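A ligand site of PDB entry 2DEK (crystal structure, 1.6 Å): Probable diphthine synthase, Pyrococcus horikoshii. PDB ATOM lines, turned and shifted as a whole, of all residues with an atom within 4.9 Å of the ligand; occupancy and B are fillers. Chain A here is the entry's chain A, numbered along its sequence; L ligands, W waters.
The backbone NH (N) of Ile 116 lies within hydrogen-bond range of an oxygen (O2) of the ligand (3.0 Å). N of Leu 166 lies within hydrogen-bond range of O5 of the ligand, at 2.8 Å. An oxygen (O4) of the ligand is in hydrogen-bond range of the backbone carbonyl oxygen (O) of Leu 166, 2.8 Å away. The backbone carbonyl oxygen (O) of Asp 87 is in hydrogen-bond range of a nitrogen (N1) of the ligand, 2.9 Å away. O of His 234 is in hydrogen-bond range of O5 of the ligand (2.9 Å). An oxygen (O1) of the ligand lies within hydrogen-bond range of the backbone NH of Asp 87 (2.9 Å). N of Ala 209 lies within hydrogen-bond range of N5 of the ligand, 3.0 Å away. N4 of the ligand sits at hydrogen-bond distance from O of Ala 209. The backbone NH (N) of Arg 208 is in hydrogen-bond range of a nitrogen (N5) of the ligand (3.5 Å). A nitrogen (N4) of the ligand is in hydrogen-bond range of the backbone carbonyl oxygen (O) of Leu 10 (3.2 Å). O1 of the ligand sits at hydrogen-bond distance from OG of Ser 115 (2.7 Å). The backbone carbonyl oxygen (O) of Val 90 sits at hydrogen-bond distance from a nitrogen (N1) of the ligand, at 2.7 Å.
The backbone carbonyl oxygen (O) of Leu 206 lies within hydrogen-bond range of the backbone NH (N) of Ile 235, 3.0 Å away. The side-chain hydroxyl (OG) of Ser 115 lies close to the backbone NH (N) of Tyr 117 (3.1 Å). O of Pro 233 lies within hydrogen-bond range of N of Arg 208, at 2.9 Å.
O of Thr 36 sits close to S1 of the ligand. Merely in contact with the ligand: Ser 37, Pro 85, Gly 86, Ala 91, Thr 92, Phe 165, Leu 206, Pro 233 and Ile 235. Hydrophobic or aromatic side chains that line the ligand: Leu 10, Val 90, Ala 91, Ile 116, Phe 165, Leu 166, Ala 209, Pro 233 and Ile 235. Of the 26 residues printed, 19 come within 4 Å of the ligand. The nearest printed residue that does not touch the ligand is Ile 168 (4.4 Å).
Water W4 bridges O4 of the ligand (2.6 Å) and O of Asp 167 (3.0 Å). Water W1 lies within hydrogen-bond range of the backbone carbonyl oxygen of Pro 85 (2.7 Å), the side-chain hydroxyl of Thr 36 (2.7 Å) and a nitrogen (N1) of the ligand (2.8 Å).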
ATOM      1  N   LEU A  10      13.300  26.454  35.648  1.00  0.00           N
ATOM      2  CA  LEU A  10      11.955  26.242  35.096  1.00  0.00           C
ATOM      3  C   LEU A  10      11.111  27.495  34.831  1.00  0.00           C
ATOM      4  O   LEU A  10      10.410  27.591  33.842  1.00  0.00           O
ATOM      5  CB  LEU A  10      11.178  25.388  36.085  1.00  0.00           C
ATOM      6  CG  LEU A  10      11.716  23.969  36.286  1.00  0.00           C
ATOM      7  CD1 LEU A  10      11.089  23.305  37.515  1.00  0.00           C
ATOM      8  CD2 LEU A  10      11.411  23.047  35.121  1.00  0.00           C
ATOM      9  N   TYR A  11      11.119  28.441  35.791  1.00  0.00           N
ATOM     10  CA  TYR A  11      10.094  29.494  35.746  1.00  0.00           C
ATOM     11  C   TYR A  11      10.629  30.938  35.858  1.00  0.00           C
ATOM     12  O   TYR A  11      10.322  31.812  35.053  1.00  0.00           O
ATOM     13  CB  TYR A  11       9.029  29.214  36.817  1.00  0.00           C
ATOM     14  CG  TYR A  11       7.930  30.228  36.793  1.00  0.00           C
ATOM     15  CD1 TYR A  11       6.966  30.209  35.778  1.00  0.00           C
ATOM     16  CD2 TYR A  11       7.768  31.122  37.850  1.00  0.00           C
ATOM     17  CE1 TYR A  11       5.871  31.054  35.832  1.00  0.00           C
ATOM     18  CE2 TYR A  11       6.669  31.973  37.898  1.00  0.00           C
ATOM     19  CZ  TYR A  11       5.733  31.953  36.893  1.00  0.00           C
ATOM     20  OH  TYR A  11       4.653  32.807  36.932  1.00  0.00           O
ATOM     21  N   THR A  36      14.710  27.864  23.228  1.00  0.00           N
ATOM     22  CA  THR A  36      14.458  26.436  23.470  1.00  0.00           C
ATOM     23  C   THR A  36      13.312  26.190  24.473  1.00  0.00           C
ATOM     24  O   THR A  36      12.770  25.098  24.575  1.00  0.00           O
ATOM     25  CB  THR A  36      15.732  25.755  24.003  1.00  0.00           C
ATOM     26  OG1 THR A  36      16.161  26.398  25.205  1.00  0.00           O
ATOM     27  CG2 THR A  36      16.846  25.801  22.965  1.00  0.00           C
ATOM     28  N   SER A  37      12.991  27.235  25.258  1.00  0.00           N
ATOM     29  CA  SER A  37      11.905  27.119  26.213  1.00  0.00           C
ATOM     30  C   SER A  37      11.415  28.490  26.657  1.00  0.00           C
ATOM     31  O   SER A  37      11.898  29.518  26.215  1.00  0.00           O
ATOM     32  CB  SER A  37      12.408  26.319  27.420  1.00  0.00           C
ATOM     33  OG  SER A  37      11.300  25.995  28.267  1.00  0.00           O
ATOM     34  N   LEU A  38      10.413  28.478  27.539  1.00  0.00           N
ATOM     35  CA  LEU A  38       9.857  29.740  28.024  1.00  0.00           C
ATOM     36  C   LEU A  38       9.898  29.803  29.555  1.00  0.00           C
ATOM     37  O   LEU A  38       9.389  28.938  30.256  1.00  0.00           O
ATOM     38  CB  LEU A  38       8.411  29.850  27.521  1.00  0.00           C
ATOM     39  CG  LEU A  38       7.660  31.068  28.051  1.00  0.00           C
ATOM     40  CD1 LEU A  38       8.236  32.387  27.513  1.00  0.00           C
ATOM     41  CD2 LEU A  38       6.185  31.063  27.666  1.00  0.00           C
ATOM     42  N   PRO A  85      17.293  28.359  29.429  1.00  0.00           N
ATOM     43  CA  PRO A  85      16.189  27.977  30.264  1.00  0.00           C
ATOM     44  C   PRO A  85      16.336  26.490  30.678  1.00  0.00           C
ATOM     45  O   PRO A  85      16.988  25.688  30.015  1.00  0.00           O
ATOM     46  CB  PRO A  85      14.914  28.204  29.470  1.00  0.00           C
ATOM     47  CG  PRO A  85      15.289  29.161  28.337  1.00  0.00           C
ATOM     48  CD  PRO A  85      16.806  28.742  28.103  1.00  0.00           C
ATOM     49  N   GLY A  86      15.737  26.165  31.834  1.00  0.00           N
ATOM     50  CA  GLY A  86      15.811  24.783  32.315  1.00  0.00           C
ATOM     51  C   GLY A  86      17.258  24.279  32.433  1.00  0.00           C
ATOM     52  O   GLY A  86      18.156  24.989  32.867  1.00  0.00           O
ATOM     53  N   ASP A  87      17.451  23.000  32.072  1.00  0.00           N
ATOM     54  CA  ASP A  87      18.796  22.450  31.953  1.00  0.00           C
ATOM     55  C   ASP A  87      19.270  22.601  30.498  1.00  0.00           C
ATOM     56  O   ASP A  87      18.545  22.301  29.554  1.00  0.00           O
ATOM     57  CB  ASP A  87      18.742  20.973  32.346  1.00  0.00           C
ATOM     58  CG  ASP A  87      20.142  20.372  32.355  1.00  0.00           C
ATOM     59  OD1 ASP A  87      20.709  20.214  31.272  1.00  0.00           O
ATOM     60  OD2 ASP A  87      20.612  19.998  33.430  1.00  0.00           O
ATOM     61  N   VAL A  90      18.974  19.379  28.137  1.00  0.00           N
ATOM     62  CA  VAL A  90      17.768  18.561  28.038  1.00  0.00           C
ATOM     63  C   VAL A  90      16.809  19.034  26.944  1.00  0.00           C
ATOM     64  O   VAL A  90      16.307  20.151  26.946  1.00  0.00           O
ATOM     65  CB  VAL A  90      17.033  18.579  29.389  1.00  0.00           C
ATOM     66  CG1 VAL A  90      15.709  17.820  29.267  1.00  0.00           C
ATOM     67  CG2 VAL A  90      17.886  17.916  30.458  1.00  0.00           C
ATOM     68  N   ALA A  91      16.580  18.138  25.952  1.00  0.00           N
ATOM     69  CA  ALA A  91      15.674  18.448  24.852  1.00  0.00           C
ATOM     70  C   ALA A  91      16.121  19.694  24.084  1.00  0.00           C
ATOM     71  O   ALA A  91      15.321  20.511  23.637  1.00  0.00           O
ATOM     72  CB  ALA A  91      14.267  18.631  25.396  1.00  0.00           C
ATOM     73  N   THR A  92      17.450  19.846  24.005  1.00  0.00           N
ATOM     74  CA  THR A  92      18.047  20.825  23.121  1.00  0.00           C
ATOM     75  C   THR A  92      19.149  20.126  22.333  1.00  0.00           C
ATOM     76  O   THR A  92      19.459  18.965  22.552  1.00  0.00           O
ATOM     77  CB  THR A  92      18.674  21.937  23.959  1.00  0.00           C
ATOM     78  OG1 THR A  92      19.876  21.441  24.559  1.00  0.00           O
ATOM     79  CG2 THR A  92      17.713  22.384  25.070  1.00  0.00           C
ATOM     80  N   PRO A 114      17.050  23.033  37.458  1.00  0.00           N
ATOM     81  CA  PRO A 114      15.798  22.273  37.397  1.00  0.00           C
ATOM     82  C   PRO A 114      15.313  22.157  35.945  1.00  0.00           C
ATOM     83  O   PRO A 114      15.290  23.144  35.212  1.00  0.00           O
ATOM     84  CB  PRO A 114      14.837  23.104  38.241  1.00  0.00           C
ATOM     85  CG  PRO A 114      15.722  23.810  39.202  1.00  0.00           C
ATOM     86  CD  PRO A 114      16.947  24.162  38.401  1.00  0.00           C
ATOM     87  N   SER A 115      14.912  20.947  35.569  1.00  0.00           N
ATOM     88  CA  SER A 115      14.439  20.672  34.215  1.00  0.00           C
ATOM     89  C   SER A 115      13.011  20.152  34.230  1.00  0.00           C
ATOM     90  O   SER A 115      12.602  19.499  35.190  1.00  0.00           O
ATOM     91  CB  SER A 115      15.342  19.624  33.560  1.00  0.00           C
ATOM     92  OG  SER A 115      14.803  19.178  32.324  1.00  0.00           O
ATOM     93  N   ILE A 116      12.251  20.444  33.176  1.00  0.00           N
ATOM     94  CA  ILE A 116      10.876  19.957  33.101  1.00  0.00           C
ATOM     95  C   ILE A 116      10.885  18.426  33.106  1.00  0.00           C
ATOM     96  O   ILE A 116       9.959  17.795  33.601  1.00  0.00           O
ATOM     97  CB  ILE A 116      10.156  20.477  31.818  1.00  0.00           C
ATOM     98  CG1 ILE A 116       8.653  20.117  31.865  1.00  0.00           C
ATOM     99  CG2 ILE A 116      10.778  19.856  30.566  1.00  0.00           C
ATOM    100  CD1 ILE A 116       7.911  20.667  33.076  1.00  0.00           C
ATOM    101  N   TYR A 117      11.977  17.843  32.597  1.00  0.00           N
ATOM    102  CA  TYR A 117      12.085  16.389  32.526  1.00  0.00           C
ATOM    103  C   TYR A 117      11.957  15.716  33.899  1.00  0.00           C
ATOM    104  O   TYR A 117      11.394  14.628  34.003  1.00  0.00           O
ATOM    105  CB  TYR A 117      13.396  15.992  31.853  1.00  0.00           C
ATOM    106  CG  TYR A 117      13.436  14.529  31.440  1.00  0.00           C
ATOM    107  CD1 TYR A 117      12.638  14.049  30.401  1.00  0.00           C
ATOM    108  CD2 TYR A 117      14.265  13.625  32.117  1.00  0.00           C
ATOM    109  CE1 TYR A 117      12.665  12.700  30.043  1.00  0.00           C
ATOM    110  CE2 TYR A 117      14.285  12.283  31.770  1.00  0.00           C
ATOM    111  CZ  TYR A 117      13.486  11.824  30.737  1.00  0.00           C
ATOM    112  OH  TYR A 117      13.507  10.490  30.396  1.00  0.00           O
ATOM    113  N   PHE A 165       6.791  16.886  25.085  1.00  0.00           N
ATOM    114  CA  PHE A 165       7.218  18.265  25.065  1.00  0.00           C
ATOM    115  C   PHE A 165       6.369  18.965  24.015  1.00  0.00           C
ATOM    116  O   PHE A 165       5.995  18.368  23.017  1.00  0.00           O
ATOM    117  CB  PHE A 165       8.706  18.349  24.635  1.00  0.00           C
ATOM    118  CG  PHE A 165       9.639  17.725  25.648  1.00  0.00           C
ATOM    119  CD1 PHE A 165      10.053  16.409  25.465  1.00  0.00           C
ATOM    120  CD2 PHE A 165      10.226  18.500  26.656  1.00  0.00           C
ATOM    121  CE1 PHE A 165      11.007  15.853  26.306  1.00  0.00           C
ATOM    122  CE2 PHE A 165      11.182  17.931  27.497  1.00  0.00           C
ATOM    123  CZ  PHE A 165      11.573  16.604  27.334  1.00  0.00           C
ATOM    124  N   LEU A 166       6.001  20.220  24.277  1.00  0.00           N
ATOM    125  CA  LEU A 166       5.189  20.907  23.281  1.00  0.00           C
ATOM    126  C   LEU A 166       5.999  21.924  22.485  1.00  0.00           C
ATOM    127  O   LEU A 166       6.997  22.465  22.939  1.00  0.00           O
ATOM    128  CB  LEU A 166       4.026  21.594  24.005  1.00  0.00           C
ATOM    129  CG  LEU A 166       3.168  20.591  24.798  1.00  0.00           C
ATOM    130  CD1 LEU A 166       1.875  21.214  25.314  1.00  0.00           C
ATOM    131  CD2 LEU A 166       2.730  19.381  23.979  1.00  0.00           C
ATOM    132  N   ASP A 167       5.543  22.164  21.231  1.00  0.00           N
ATOM    133  CA  ASP A 167       6.273  23.027  20.309  1.00  0.00           C
ATOM    134  C   ASP A 167       6.381  24.473  20.797  1.00  0.00           C
ATOM    135  O   ASP A 167       5.571  24.968  21.579  1.00  0.00           O
ATOM    136  CB  ASP A 167       5.575  22.988  18.951  1.00  0.00           C
ATOM    137  CG  ASP A 167       6.573  23.163  17.820  1.00  0.00           C
ATOM    138  OD1 ASP A 167       7.718  23.520  18.104  1.00  0.00           O
ATOM    139  OD2 ASP A 167       6.204  22.962  16.667  1.00  0.00           O
ATOM    140  N   ILE A 168       7.462  25.123  20.332  1.00  0.00           N
ATOM    141  CA  ILE A 168       7.673  26.534  20.576  1.00  0.00           C
ATOM    142  C   ILE A 168       8.327  27.203  19.381  1.00  0.00           C
ATOM    143  O   ILE A 168       9.211  26.668  18.726  1.00  0.00           O
ATOM    144  CB  ILE A 168       8.566  26.678  21.812  1.00  0.00           C
ATOM    145  CG1 ILE A 168       8.940  28.143  22.041  1.00  0.00           C
ATOM    146  CG2 ILE A 168       9.868  25.882  21.622  1.00  0.00           C
ATOM    147  CD1 ILE A 168       9.769  28.357  23.305  1.00  0.00           C
ATOM    148  N   LEU A 206       0.616  19.729  32.877  1.00  0.00           N
ATOM    149  CA  LEU A 206       1.421  20.466  33.840  1.00  0.00           C
ATOM    150  C   LEU A 206       1.801  21.770  33.165  1.00  0.00           C
ATOM    151  O   LEU A 206       2.465  21.787  32.129  1.00  0.00           O
ATOM    152  CB  LEU A 206       2.683  19.677  34.218  1.00  0.00           C
ATOM    153  CG  LEU A 206       3.689  20.422  35.114  1.00  0.00           C
ATOM    154  CD1 LEU A 206       2.995  20.902  36.382  1.00  0.00           C
ATOM    155  CD2 LEU A 206       4.848  19.486  35.461  1.00  0.00           C
ATOM    156  N   ALA A 207       1.358  22.874  33.749  1.00  0.00           N
ATOM    157  CA  ALA A 207       1.637  24.195  33.195  1.00  0.00           C
ATOM    158  C   ALA A 207       2.409  25.056  34.175  1.00  0.00           C
ATOM    159  O   ALA A 207       2.064  25.137  35.354  1.00  0.00           O
ATOM    160  CB  ALA A 207       0.333  24.876  32.816  1.00  0.00           C
ATOM    161  N   ARG A 208       3.463  25.692  33.669  1.00  0.00           N
ATOM    162  CA  ARG A 208       4.299  26.585  34.460  1.00  0.00           C
ATOM    163  C   ARG A 208       4.934  25.935  35.686  1.00  0.00           C
ATOM    164  O   ARG A 208       4.854  26.458  36.809  1.00  0.00           O
ATOM    165  CB  ARG A 208       3.487  27.817  34.861  1.00  0.00           C
ATOM    166  CG  ARG A 208       2.835  28.536  33.666  1.00  0.00           C
ATOM    167  CD  ARG A 208       1.991  29.716  34.125  1.00  0.00           C
ATOM    168  NE  ARG A 208       1.060  29.320  35.188  1.00  0.00           N
ATOM    169  CZ  ARG A 208      -0.027  28.568  35.006  1.00  0.00           C
ATOM    170  NH1 ARG A 208      -0.356  28.141  33.798  1.00  0.00           N
ATOM    171  NH2 ARG A 208      -0.768  28.230  36.041  1.00  0.00           N
ATOM    172  N   ALA A 209       5.569  24.782  35.481  1.00  0.00           N
ATOM    173  CA  ALA A 209       6.284  24.155  36.575  1.00  0.00           C
ATOM    174  C   ALA A 209       7.371  25.096  37.009  1.00  0.00           C
ATOM    175  O   ALA A 209       7.898  25.860  36.219  1.00  0.00           O
ATOM    176  CB  ALA A 209       6.881  22.848  36.069  1.00  0.00           C
ATOM    177  N   PRO A 233       4.545  28.047  29.707  1.00  0.00           N
ATOM    178  CA  PRO A 233       4.623  26.799  28.935  1.00  0.00           C
ATOM    179  C   PRO A 233       3.796  25.658  29.535  1.00  0.00           C
ATOM    180  O   PRO A 233       3.528  25.630  30.730  1.00  0.00           O
ATOM    181  CB  PRO A 233       6.108  26.484  28.954  1.00  0.00           C
ATOM    182  CG  PRO A 233       6.496  26.912  30.337  1.00  0.00           C
ATOM    183  CD  PRO A 233       5.777  28.243  30.491  1.00  0.00           C
ATOM    184  N   HIS A 234       3.410  24.719  28.672  1.00  0.00           N
ATOM    185  CA  HIS A 234       2.630  23.564  29.081  1.00  0.00           C
ATOM    186  C   HIS A 234       3.338  22.306  28.613  1.00  0.00           C
ATOM    187  O   HIS A 234       4.101  22.342  27.655  1.00  0.00           O
ATOM    188  CB  HIS A 234       1.256  23.507  28.392  1.00  0.00           C
ATOM    189  CG  HIS A 234       0.331  24.627  28.753  1.00  0.00           C
ATOM    190  ND1 HIS A 234      -0.948  24.719  28.223  1.00  0.00           N
ATOM    191  CD2 HIS A 234       0.459  25.667  29.595  1.00  0.00           C
ATOM    192  CE1 HIS A 234      -1.552  25.767  28.730  1.00  0.00           C
ATOM    193  NE2 HIS A 234      -0.721  26.366  29.563  1.00  0.00           N
ATOM    194  N   ILE A 235       3.061  21.212  29.289  1.00  0.00           N
ATOM    195  CA  ILE A 235       3.585  19.926  28.875  1.00  0.00           C
ATOM    196  C   ILE A 235       2.394  18.982  29.009  1.00  0.00           C
ATOM    197  O   ILE A 235       1.518  19.196  29.850  1.00  0.00           O
ATOM    198  CB  ILE A 235       4.799  19.485  29.759  1.00  0.00           C
ATOM    199  CG1 ILE A 235       5.571  18.399  29.027  1.00  0.00           C
ATOM    200  CG2 ILE A 235       4.328  19.016  31.123  1.00  0.00           C
ATOM    201  CD1 ILE A 235       7.068  18.446  29.304  1.00  0.00           C
HETATM  202  N1  LIG L   1      15.860  22.361  28.393  1.00  0.00           N
HETATM  203  C1  LIG L   1      14.525  22.586  28.963  1.00  0.00           C
HETATM  204  C2  LIG L   1      13.460  21.905  28.103  1.00  0.00           C
HETATM  205  C3  LIG L   1      13.455  22.417  26.658  1.00  0.00           C
HETATM  206  S1  LIG L   1      12.069  21.710  25.694  1.00  0.00           S
HETATM  207  C4  LIG L   1      14.457  21.981  30.365  1.00  0.00           C
HETATM  208  O1  LIG L   1      15.409  21.339  30.811  1.00  0.00           O
HETATM  209  O2  LIG L   1      13.443  22.117  31.050  1.00  0.00           O
HETATM  210  C5  LIG L   1      10.823  23.032  25.928  1.00  0.00           C
HETATM  211  C6  LIG L   1       9.439  22.504  26.328  1.00  0.00           C
HETATM  212  O3  LIG L   1       9.453  21.873  27.610  1.00  0.00           O
HETATM  213  C7  LIG L   1       8.417  23.636  26.459  1.00  0.00           C
HETATM  214  O4  LIG L   1       7.916  23.975  25.160  1.00  0.00           O
HETATM  215  C8  LIG L   1       7.342  22.885  27.243  1.00  0.00           C
HETATM  216  O5  LIG L   1       6.683  21.933  26.410  1.00  0.00           O
HETATM  217  C9  LIG L   1       8.210  22.165  28.280  1.00  0.00           C
HETATM  218  N2  LIG L   1       8.490  23.054  29.428  1.00  0.00           N
HETATM  219  C10 LIG L   1       9.647  23.671  29.695  1.00  0.00           C
HETATM  220  N3  LIG L   1       9.563  24.316  30.846  1.00  0.00           N
HETATM  221  C11 LIG L   1       8.342  24.118  31.340  1.00  0.00           C
HETATM  222  C12 LIG L   1       7.667  24.526  32.483  1.00  0.00           C
HETATM  223  N4  LIG L   1       8.275  25.314  33.372  1.00  0.00           N
HETATM  224  N5  LIG L   1       6.399  24.130  32.670  1.00  0.00           N
HETATM  225  C13 LIG L   1       5.778  23.369  31.784  1.00  0.00           C
HETATM  226  N6  LIG L   1       6.384  22.966  30.686  1.00  0.00           N
HETATM  227  C14 LIG L   1       7.659  23.324  30.430  1.00  0.00           C
HETATM  228  O   HOH W   1      16.188  24.984  27.553  1.00  0.00           O
HETATM  229  O   HOH W   2      12.374  24.646  31.775  1.00  0.00           O
HETATM  230  O   HOH W   3      11.829  26.871  30.916  1.00  0.00           O
HETATM  231  O   HOH W   4       6.018  25.652  24.425  1.00  0.00           O
